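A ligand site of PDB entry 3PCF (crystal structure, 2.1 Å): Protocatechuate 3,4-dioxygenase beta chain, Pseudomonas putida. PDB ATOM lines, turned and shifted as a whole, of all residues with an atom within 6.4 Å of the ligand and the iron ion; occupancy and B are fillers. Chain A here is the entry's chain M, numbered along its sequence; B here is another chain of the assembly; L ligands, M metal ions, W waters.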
ATOM      1  N   TYR A  24     -13.042 -28.315 -18.366  1.00  0.00           N
ATOM      2  CA  TYR A  24     -12.638 -27.835 -17.030  1.00  0.00           C
ATOM      3  C   TYR A  24     -14.034 -27.518 -16.432  1.00  0.00           C
ATOM      4  O   TYR A  24     -14.553 -26.389 -16.617  1.00  0.00           O
ATOM      5  CB  TYR A  24     -11.806 -26.534 -17.100  1.00  0.00           C
ATOM      6  CG  TYR A  24     -11.469 -26.039 -15.702  1.00  0.00           C
ATOM      7  CD1 TYR A  24     -11.509 -26.889 -14.598  1.00  0.00           C
ATOM      8  CD2 TYR A  24     -11.142 -24.721 -15.465  1.00  0.00           C
ATOM      9  CE1 TYR A  24     -11.155 -26.458 -13.326  1.00  0.00           C
ATOM     10  CE2 TYR A  24     -10.753 -24.270 -14.200  1.00  0.00           C
ATOM     11  CZ  TYR A  24     -10.799 -25.149 -13.125  1.00  0.00           C
ATOM     12  OH  TYR A  24     -10.485 -24.629 -11.896  1.00  0.00           O
ATOM     13  N   THR A  26     -15.536 -26.902 -13.569  1.00  0.00           N
ATOM     14  CA  THR A  26     -15.940 -25.793 -12.699  1.00  0.00           C
ATOM     15  C   THR A  26     -16.250 -24.528 -13.478  1.00  0.00           C
ATOM     16  O   THR A  26     -17.072 -23.766 -13.007  1.00  0.00           O
ATOM     17  CB  THR A  26     -14.940 -25.470 -11.543  1.00  0.00           C
ATOM     18  OG1 THR A  26     -14.679 -26.748 -10.932  1.00  0.00           O
ATOM     19  CG2 THR A  26     -15.572 -24.593 -10.432  1.00  0.00           C
ATOM     20  N   TRP A 100       2.636 -20.384  -4.397  1.00  0.00           N
ATOM     21  CA  TRP A 100       2.077 -21.435  -3.556  1.00  0.00           C
ATOM     22  C   TRP A 100       2.014 -22.706  -4.419  1.00  0.00           C
ATOM     23  O   TRP A 100       1.907 -22.703  -5.649  1.00  0.00           O
ATOM     24  CB  TRP A 100       0.823 -21.020  -2.803  1.00  0.00           C
ATOM     25  CG  TRP A 100      -0.423 -21.030  -3.631  1.00  0.00           C
ATOM     26  CD1 TRP A 100      -1.315 -22.032  -3.767  1.00  0.00           C
ATOM     27  CD2 TRP A 100      -0.888 -19.965  -4.492  1.00  0.00           C
ATOM     28  NE1 TRP A 100      -2.345 -21.678  -4.595  1.00  0.00           N
ATOM     29  CE2 TRP A 100      -2.113 -20.414  -5.039  1.00  0.00           C
ATOM     30  CE3 TRP A 100      -0.444 -18.706  -4.755  1.00  0.00           C
ATOM     31  CZ2 TRP A 100      -2.870 -19.664  -5.943  1.00  0.00           C
ATOM     32  CZ3 TRP A 100      -1.171 -17.947  -5.679  1.00  0.00           C
ATOM     33  CH2 TRP A 100      -2.328 -18.414  -6.279  1.00  0.00           C
ATOM     34  N   GLN A 101       2.219 -23.782  -3.730  1.00  0.00           N
ATOM     35  CA  GLN A 101       2.266 -25.134  -4.344  1.00  0.00           C
ATOM     36  C   GLN A 101       2.048 -26.212  -3.276  1.00  0.00           C
ATOM     37  O   GLN A 101       1.975 -25.924  -2.067  1.00  0.00           O
ATOM     38  CB  GLN A 101       3.714 -25.307  -4.911  1.00  0.00           C
ATOM     39  CG  GLN A 101       4.769 -25.113  -3.842  1.00  0.00           C
ATOM     40  CD  GLN A 101       6.166 -25.615  -4.141  1.00  0.00           C
ATOM     41  OE1 GLN A 101       7.082 -24.877  -4.488  1.00  0.00           O
ATOM     42  NE2 GLN A 101       6.382 -26.944  -3.983  1.00  0.00           N
ATOM     43  N   ALA A 102       1.956 -27.428  -3.773  1.00  0.00           N
ATOM     44  CA  ALA A 102       1.830 -28.639  -2.964  1.00  0.00           C
ATOM     45  C   ALA A 102       3.271 -29.110  -2.657  1.00  0.00           C
ATOM     46  O   ALA A 102       4.327 -28.563  -3.096  1.00  0.00           O
ATOM     47  CB  ALA A 102       1.161 -29.752  -3.835  1.00  0.00           C
ATOM     48  N   TYR A 108      -1.389 -30.604  -0.464  1.00  0.00           N
ATOM     49  CA  TYR A 108      -1.463 -29.178  -0.130  1.00  0.00           C
ATOM     50  C   TYR A 108      -1.774 -29.014   1.364  1.00  0.00           C
ATOM     51  O   TYR A 108      -2.604 -29.771   1.887  1.00  0.00           O
ATOM     52  CB  TYR A 108      -2.489 -28.414  -0.924  1.00  0.00           C
ATOM     53  CG  TYR A 108      -2.227 -27.995  -2.317  1.00  0.00           C
ATOM     54  CD1 TYR A 108      -1.492 -26.849  -2.648  1.00  0.00           C
ATOM     55  CD2 TYR A 108      -2.748 -28.759  -3.374  1.00  0.00           C
ATOM     56  CE1 TYR A 108      -1.280 -26.474  -3.987  1.00  0.00           C
ATOM     57  CE2 TYR A 108      -2.540 -28.399  -4.707  1.00  0.00           C
ATOM     58  CZ  TYR A 108      -1.843 -27.250  -5.003  1.00  0.00           C
ATOM     59  OH  TYR A 108      -1.722 -26.920  -6.307  1.00  0.00           O
ATOM     60  N   TYR A 147      -1.066 -34.255  -8.842  1.00  0.00           N
ATOM     61  CA  TYR A 147      -2.147 -34.746  -7.932  1.00  0.00           C
ATOM     62  C   TYR A 147      -3.475 -34.855  -8.659  1.00  0.00           C
ATOM     63  O   TYR A 147      -3.778 -34.145  -9.612  1.00  0.00           O
ATOM     64  CB  TYR A 147      -2.297 -33.978  -6.631  1.00  0.00           C
ATOM     65  CG  TYR A 147      -2.656 -32.535  -6.952  1.00  0.00           C
ATOM     66  CD1 TYR A 147      -1.630 -31.651  -7.157  1.00  0.00           C
ATOM     67  CD2 TYR A 147      -3.979 -32.131  -7.068  1.00  0.00           C
ATOM     68  CE1 TYR A 147      -1.894 -30.314  -7.476  1.00  0.00           C
ATOM     69  CE2 TYR A 147      -4.275 -30.822  -7.383  1.00  0.00           C
ATOM     70  CZ  TYR A 147      -3.226 -29.914  -7.593  1.00  0.00           C
ATOM     71  OH  TYR A 147      -3.416 -28.601  -7.873  1.00  0.00           O
ATOM     72  N   TRP A 149      -7.557 -34.863  -9.158  1.00  0.00           N
ATOM     73  CA  TRP A 149      -8.627 -33.860  -8.824  1.00  0.00           C
ATOM     74  C   TRP A 149      -9.929 -34.347  -9.440  1.00  0.00           C
ATOM     75  O   TRP A 149      -9.953 -34.989 -10.510  1.00  0.00           O
ATOM     76  CB  TRP A 149      -8.183 -32.470  -9.194  1.00  0.00           C
ATOM     77  CG  TRP A 149      -7.925 -32.222 -10.639  1.00  0.00           C
ATOM     78  CD1 TRP A 149      -6.927 -32.768 -11.444  1.00  0.00           C
ATOM     79  CD2 TRP A 149      -8.613 -31.275 -11.476  1.00  0.00           C
ATOM     80  NE1 TRP A 149      -7.006 -32.277 -12.724  1.00  0.00           N
ATOM     81  CE2 TRP A 149      -8.012 -31.335 -12.761  1.00  0.00           C
ATOM     82  CE3 TRP A 149      -9.664 -30.395 -11.235  1.00  0.00           C
ATOM     83  CZ2 TRP A 149      -8.448 -30.539 -13.813  1.00  0.00           C
ATOM     84  CZ3 TRP A 149     -10.111 -29.625 -12.294  1.00  0.00           C
ATOM     85  CH2 TRP A 149      -9.502 -29.677 -13.555  1.00  0.00           C
ATOM     86  N   ARG A 150     -11.015 -33.995  -8.772  1.00  0.00           N
ATOM     87  CA  ARG A 150     -12.360 -34.414  -9.206  1.00  0.00           C
ATOM     88  C   ARG A 150     -12.848 -33.546 -10.336  1.00  0.00           C
ATOM     89  O   ARG A 150     -13.500 -32.524 -10.103  1.00  0.00           O
ATOM     90  CB  ARG A 150     -13.336 -34.578  -8.045  1.00  0.00           C
ATOM     91  CG  ARG A 150     -12.901 -35.566  -6.948  1.00  0.00           C
ATOM     92  CD  ARG A 150     -13.895 -36.598  -6.508  1.00  0.00           C
ATOM     93  NE  ARG A 150     -13.744 -37.905  -7.169  1.00  0.00           N
ATOM     94  CZ  ARG A 150     -13.696 -39.126  -6.586  1.00  0.00           C
ATOM     95  NH1 ARG A 150     -13.833 -39.309  -5.256  1.00  0.00           N
ATOM     96  NH2 ARG A 150     -13.308 -40.198  -7.318  1.00  0.00           N
ATOM     97  N   ARG A 157      -3.400 -33.078 -12.324  1.00  0.00           N
ATOM     98  CA  ARG A 157      -2.742 -31.787 -12.709  1.00  0.00           C
ATOM     99  C   ARG A 157      -1.231 -32.181 -12.825  1.00  0.00           C
ATOM    100  O   ARG A 157      -0.735 -32.868 -11.934  1.00  0.00           O
ATOM    101  CB  ARG A 157      -2.764 -30.753 -11.556  1.00  0.00           C
ATOM    102  CG  ARG A 157      -4.081 -30.295 -10.984  1.00  0.00           C
ATOM    103  CD  ARG A 157      -4.948 -29.621 -12.029  1.00  0.00           C
ATOM    104  NE  ARG A 157      -4.174 -28.885 -13.037  1.00  0.00           N
ATOM    105  CZ  ARG A 157      -3.529 -27.740 -12.858  1.00  0.00           C
ATOM    106  NH1 ARG A 157      -3.511 -27.123 -11.690  1.00  0.00           N
ATOM    107  NH2 ARG A 157      -2.962 -27.163 -13.973  1.00  0.00           N
ATOM    108  N   HIS A 160       2.958 -28.382 -10.651  1.00  0.00           N
ATOM    109  CA  HIS A 160       2.883 -26.903 -11.004  1.00  0.00           C
ATOM    110  C   HIS A 160       2.987 -26.059  -9.730  1.00  0.00           C
ATOM    111  O   HIS A 160       2.721 -26.565  -8.659  1.00  0.00           O
ATOM    112  CB  HIS A 160       1.491 -26.598 -11.702  1.00  0.00           C
ATOM    113  CG  HIS A 160       0.398 -26.814 -10.727  1.00  0.00           C
ATOM    114  ND1 HIS A 160      -0.188 -28.034 -10.441  1.00  0.00           N
ATOM    115  CD2 HIS A 160      -0.188 -25.924  -9.889  1.00  0.00           C
ATOM    116  CE1 HIS A 160      -1.123 -27.876  -9.509  1.00  0.00           C
ATOM    117  NE2 HIS A 160      -1.113 -26.585  -9.140  1.00  0.00           N
ATOM    118  N   HIS A 162       1.768 -22.301  -8.359  1.00  0.00           N
ATOM    119  CA  HIS A 162       0.751 -21.214  -8.592  1.00  0.00           C
ATOM    120  C   HIS A 162       1.509 -19.893  -8.356  1.00  0.00           C
ATOM    121  O   HIS A 162       2.181 -19.851  -7.293  1.00  0.00           O
ATOM    122  CB  HIS A 162      -0.327 -21.255  -7.427  1.00  0.00           C
ATOM    123  CG  HIS A 162      -1.224 -22.436  -7.724  1.00  0.00           C
ATOM    124  ND1 HIS A 162      -2.318 -22.365  -8.571  1.00  0.00           N
ATOM    125  CD2 HIS A 162      -1.192 -23.701  -7.238  1.00  0.00           C
ATOM    126  CE1 HIS A 162      -2.876 -23.543  -8.662  1.00  0.00           C
ATOM    127  NE2 HIS A 162      -2.226 -24.356  -7.864  1.00  0.00           N
ATOM    128  N   GLN A 177       0.150 -20.124 -13.519  1.00  0.00           N
ATOM    129  CA  GLN A 177       0.703 -21.426 -12.960  1.00  0.00           C
ATOM    130  C   GLN A 177       1.916 -21.763 -13.823  1.00  0.00           C
ATOM    131  O   GLN A 177       1.910 -21.555 -15.028  1.00  0.00           O
ATOM    132  CB  GLN A 177      -0.365 -22.533 -13.042  1.00  0.00           C
ATOM    133  CG  GLN A 177      -1.623 -22.400 -12.229  1.00  0.00           C
ATOM    134  CD  GLN A 177      -2.567 -23.558 -12.157  1.00  0.00           C
ATOM    135  OE1 GLN A 177      -2.153 -24.774 -12.106  1.00  0.00           O
ATOM    136  NE2 GLN A 177      -3.889 -23.300 -12.088  1.00  0.00           N
ATOM    137  N   TYR A 179       4.480 -24.642 -15.006  1.00  0.00           N
ATOM    138  CA  TYR A 179       4.547 -26.114 -15.248  1.00  0.00           C
ATOM    139  C   TYR A 179       6.046 -26.390 -15.516  1.00  0.00           C
ATOM    140  O   TYR A 179       6.676 -25.389 -15.916  1.00  0.00           O
ATOM    141  CB  TYR A 179       3.718 -26.429 -16.520  1.00  0.00           C
ATOM    142  CG  TYR A 179       2.253 -26.087 -16.225  1.00  0.00           C
ATOM    143  CD1 TYR A 179       1.566 -26.836 -15.258  1.00  0.00           C
ATOM    144  CD2 TYR A 179       1.605 -25.023 -16.840  1.00  0.00           C
ATOM    145  CE1 TYR A 179       0.223 -26.545 -14.946  1.00  0.00           C
ATOM    146  CE2 TYR A 179       0.299 -24.718 -16.516  1.00  0.00           C
ATOM    147  CZ  TYR A 179      -0.390 -25.457 -15.578  1.00  0.00           C
ATOM    148  OH  TYR A 179      -1.703 -25.226 -15.287  1.00  0.00           O
ATOM    149  N   ILE A 191      -7.190 -27.882 -17.517  1.00  0.00           N
ATOM    150  CA  ILE A 191      -6.877 -26.494 -17.068  1.00  0.00           C
ATOM    151  C   ILE A 191      -5.837 -25.890 -17.992  1.00  0.00           C
ATOM    152  O   ILE A 191      -5.850 -24.719 -18.414  1.00  0.00           O
ATOM    153  CB  ILE A 191      -6.485 -26.411 -15.582  1.00  0.00           C
ATOM    154  CG1 ILE A 191      -7.774 -26.668 -14.699  1.00  0.00           C
ATOM    155  CG2 ILE A 191      -5.744 -25.151 -15.164  1.00  0.00           C
ATOM    156  CD1 ILE A 191      -7.459 -26.593 -13.167  1.00  0.00           C
ATOM    157  N   THR B  12      -6.315 -20.208 -13.623  1.00  0.00           N
ATOM    158  CA  THR B  12      -7.198 -20.147 -12.441  1.00  0.00           C
ATOM    159  C   THR B  12      -6.292 -20.132 -11.206  1.00  0.00           C
ATOM    160  O   THR B  12      -5.235 -20.778 -11.207  1.00  0.00           O
ATOM    161  CB  THR B  12      -8.113 -21.411 -12.395  1.00  0.00           C
ATOM    162  OG1 THR B  12      -9.020 -21.313 -11.284  1.00  0.00           O
ATOM    163  CG2 THR B  12      -7.275 -22.738 -12.265  1.00  0.00           C
ATOM    164  N   ALA B  13      -6.767 -19.486 -10.148  1.00  0.00           N
ATOM    165  CA  ALA B  13      -6.091 -19.411  -8.876  1.00  0.00           C
ATOM    166  C   ALA B  13      -6.173 -20.795  -8.176  1.00  0.00           C
ATOM    167  O   ALA B  13      -5.289 -21.032  -7.322  1.00  0.00           O
ATOM    168  CB  ALA B  13      -6.608 -18.296  -8.015  1.00  0.00           C
ATOM    169  N   GLY B  14      -7.172 -21.564  -8.526  1.00  0.00           N
ATOM    170  CA  GLY B  14      -7.434 -22.878  -7.948  1.00  0.00           C
ATOM    171  C   GLY B  14      -8.086 -22.750  -6.564  1.00  0.00           C
ATOM    172  O   GLY B  14      -8.080 -21.674  -5.957  1.00  0.00           O
ATOM    173  N   PRO B  15      -8.559 -23.886  -6.061  1.00  0.00           N
ATOM    174  CA  PRO B  15      -9.218 -23.968  -4.753  1.00  0.00           C
ATOM    175  C   PRO B  15      -8.351 -23.651  -3.568  1.00  0.00           C
ATOM    176  O   PRO B  15      -8.852 -23.282  -2.489  1.00  0.00           O
ATOM    177  CB  PRO B  15      -9.725 -25.460  -4.715  1.00  0.00           C
ATOM    178  CG  PRO B  15      -8.688 -26.152  -5.580  1.00  0.00           C
ATOM    179  CD  PRO B  15      -8.573 -25.191  -6.760  1.00  0.00           C
ATOM    180  N   TYR B  16      -7.030 -23.732  -3.708  1.00  0.00           N
ATOM    181  CA  TYR B  16      -6.080 -23.507  -2.610  1.00  0.00           C
ATOM    182  C   TYR B  16      -5.400 -22.177  -2.607  1.00  0.00           C
ATOM    183  O   TYR B  16      -4.286 -22.048  -1.973  1.00  0.00           O
ATOM    184  CB  TYR B  16      -5.050 -24.686  -2.597  1.00  0.00           C
ATOM    185  CG  TYR B  16      -5.781 -26.025  -2.609  1.00  0.00           C
ATOM    186  CD1 TYR B  16      -6.802 -26.246  -1.683  1.00  0.00           C
ATOM    187  CD2 TYR B  16      -5.542 -26.982  -3.577  1.00  0.00           C
ATOM    188  CE1 TYR B  16      -7.498 -27.453  -1.657  1.00  0.00           C
ATOM    189  CE2 TYR B  16      -6.223 -28.193  -3.585  1.00  0.00           C
ATOM    190  CZ  TYR B  16      -7.187 -28.425  -2.615  1.00  0.00           C
ATOM    191  OH  TYR B  16      -7.930 -29.589  -2.677  1.00  0.00           O
ATOM    192  N   ARG B 133     -11.428 -20.937  -8.246  1.00  0.00           N
ATOM    193  CA  ARG B 133     -11.280 -22.114  -9.118  1.00  0.00           C
ATOM    194  C   ARG B 133     -12.544 -22.022 -10.060  1.00  0.00           C
ATOM    195  O   ARG B 133     -13.605 -21.600  -9.593  1.00  0.00           O
ATOM    196  CB  ARG B 133     -11.360 -23.458  -8.395  1.00  0.00           C
ATOM    197  CG  ARG B 133     -12.447 -23.597  -7.397  1.00  0.00           C
ATOM    198  CD  ARG B 133     -12.454 -24.966  -6.772  1.00  0.00           C
ATOM    199  NE  ARG B 133     -13.433 -25.853  -7.254  1.00  0.00           N
ATOM    200  CZ  ARG B 133     -14.630 -26.143  -6.683  1.00  0.00           C
ATOM    201  NH1 ARG B 133     -15.130 -25.613  -5.596  1.00  0.00           N
ATOM    202  NH2 ARG B 133     -15.260 -27.196  -7.234  1.00  0.00           N
ATOM    203  N   GLY B 134     -12.283 -22.380 -11.274  1.00  0.00           N
ATOM    204  CA  GLY B 134     -13.295 -22.361 -12.323  1.00  0.00           C
ATOM    205  C   GLY B 134     -13.160 -21.033 -13.086  1.00  0.00           C
ATOM    206  O   GLY B 134     -13.758 -21.019 -14.169  1.00  0.00           O
HETATM  207  C1  LIG L   1      -8.274 -27.186  -9.254  1.00  0.00           C
HETATM  208  C2  LIG L   1      -7.600 -26.145  -9.939  1.00  0.00           C
HETATM  209  C3  LIG L   1      -6.230 -26.016  -9.808  1.00  0.00           C
HETATM  210  F1  LIG L   1      -5.578 -25.006 -10.437  1.00  0.00           F
HETATM  211  C4  LIG L   1      -5.502 -26.982  -9.094  1.00  0.00           C
HETATM  212  O1  LIG L   1      -4.137 -26.812  -9.023  1.00  0.00           O
HETATM  213  C5  LIG L   1      -6.160 -28.009  -8.427  1.00  0.00           C
HETATM  214  C6  LIG L   1      -7.554 -28.113  -8.528  1.00  0.00           C
HETATM  215  C7  LIG L   1      -9.787 -27.249  -9.374  1.00  0.00           C
HETATM  216  O2  LIG L   1     -10.403 -26.450 -10.085  1.00  0.00           O
HETATM  217  O3  LIG L   1     -10.409 -28.124  -8.820  1.00  0.00           O
HETATM  218 FE    FE M   1      -2.873 -26.518  -7.645  1.00  0.00          FE
HETATM  219  O   HOH W   1      -4.640 -25.893  -6.649  1.00  0.00           O
HETATM  220  O   HOH W   2     -12.735 -27.594  -9.711  1.00  0.00           O
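NH1 of Arg 157 sits close to O1 of the ligand (2.8 Å). The side-chain hydroxyl (OH) of Tyr 24 is in hydrogen-bond range of an oxygen (O2) of the ligand, 2.6 Å away.
Within 4 Å of the iron ion: Tyr 108, Tyr 147, His 160 and His 162.
Water W2 lies within hydrogen-bond range of the side-chain hydroxyl (OG1) of Thr 26 (2.4 Å), an oxygen (O3) of the ligand (2.5 Å) and the guanidinium group (NE) of Arg 133 of chain B (3.1 Å).
The iron ion is bound by the side-chain hydroxyl (OH) of Tyr 108 (1.8 Å), an oxygen (O1) of the ligand (1.9 Å), water W1 (2.1 Å), the side-chain hydroxyl (OH) of Tyr 147 (2.2 Å), a ring nitrogen (NE2) of His 162 (2.3 Å) and a ring nitrogen (NE2) of His 160 (2.3 Å).
A fluorine (F1) of the ligand sits close to the side-chain amide nitrogen (NE2) of Gln 177, 2.9 Å away. CE3 of Trp 149 touches O3 of the ligand (3.4 Å). CD1 of Ile 191 touches C2 of the ligand, at 3.3 Å. Thr 12 of chain B touches the ligand. Gly 14 of chain B touches the ligand. Pro 15 of chain B touches the ligand (CD to C1, 3.2 Å). CB of Arg 133 of chain B touches O2 of the ligand, 3.6 Å away. Hydrophobic or aromatic side chains within 4 Å of the ligand: Tyr 24, Tyr 147, Trp 149, His 160, His 162, Ile 191 and Pro 15 of chain B. Within 4 Å of the ligand: Tyr 24, Tyr 108, Tyr 147, Trp 149, Arg 157, His 160, His 162, Gln 177, Ile 191, Thr 12 of chain B, Gly 14 of chain B, Pro 15 of chain B and Arg 133 of chain B.
The side-chain amide nitrogen (NE2) of Gln 177 lies within hydrogen-bond range of the backbone carbonyl oxygen (O) of Thr 12 of chain B (3.0 Å). The backbone NH (N) of Gly 14 of chain B sits close to the side-chain hydroxyl (OG1) of Thr 12 of chain B (3.3 Å). The backbone NH of His 162 lies within hydrogen-bond range of the backbone carbonyl oxygen of Trp 100, at 2.7 Å. The side-chain hydroxyl of Tyr 179 sits at hydrogen-bond distance from the guanidinium group of Arg 157 (2.7 Å). The backbone carbonyl oxygen (O) of Ala 13 of chain B sits at hydrogen-bond distance from a ring nitrogen (ND1) of His 162 (3.5 Å). OE1 of Gln 177 sits at hydrogen-bond distance from NH1 of Arg 157, at 2.7 Å. N of Arg 157 is in hydrogen-bond range of O of Tyr 147, at 2.9 Å. The side-chain hydroxyl of Thr 12 of chain B lies within hydrogen-bond range of the backbone NH of Gly 134 of chain B, at 3.4 Å.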
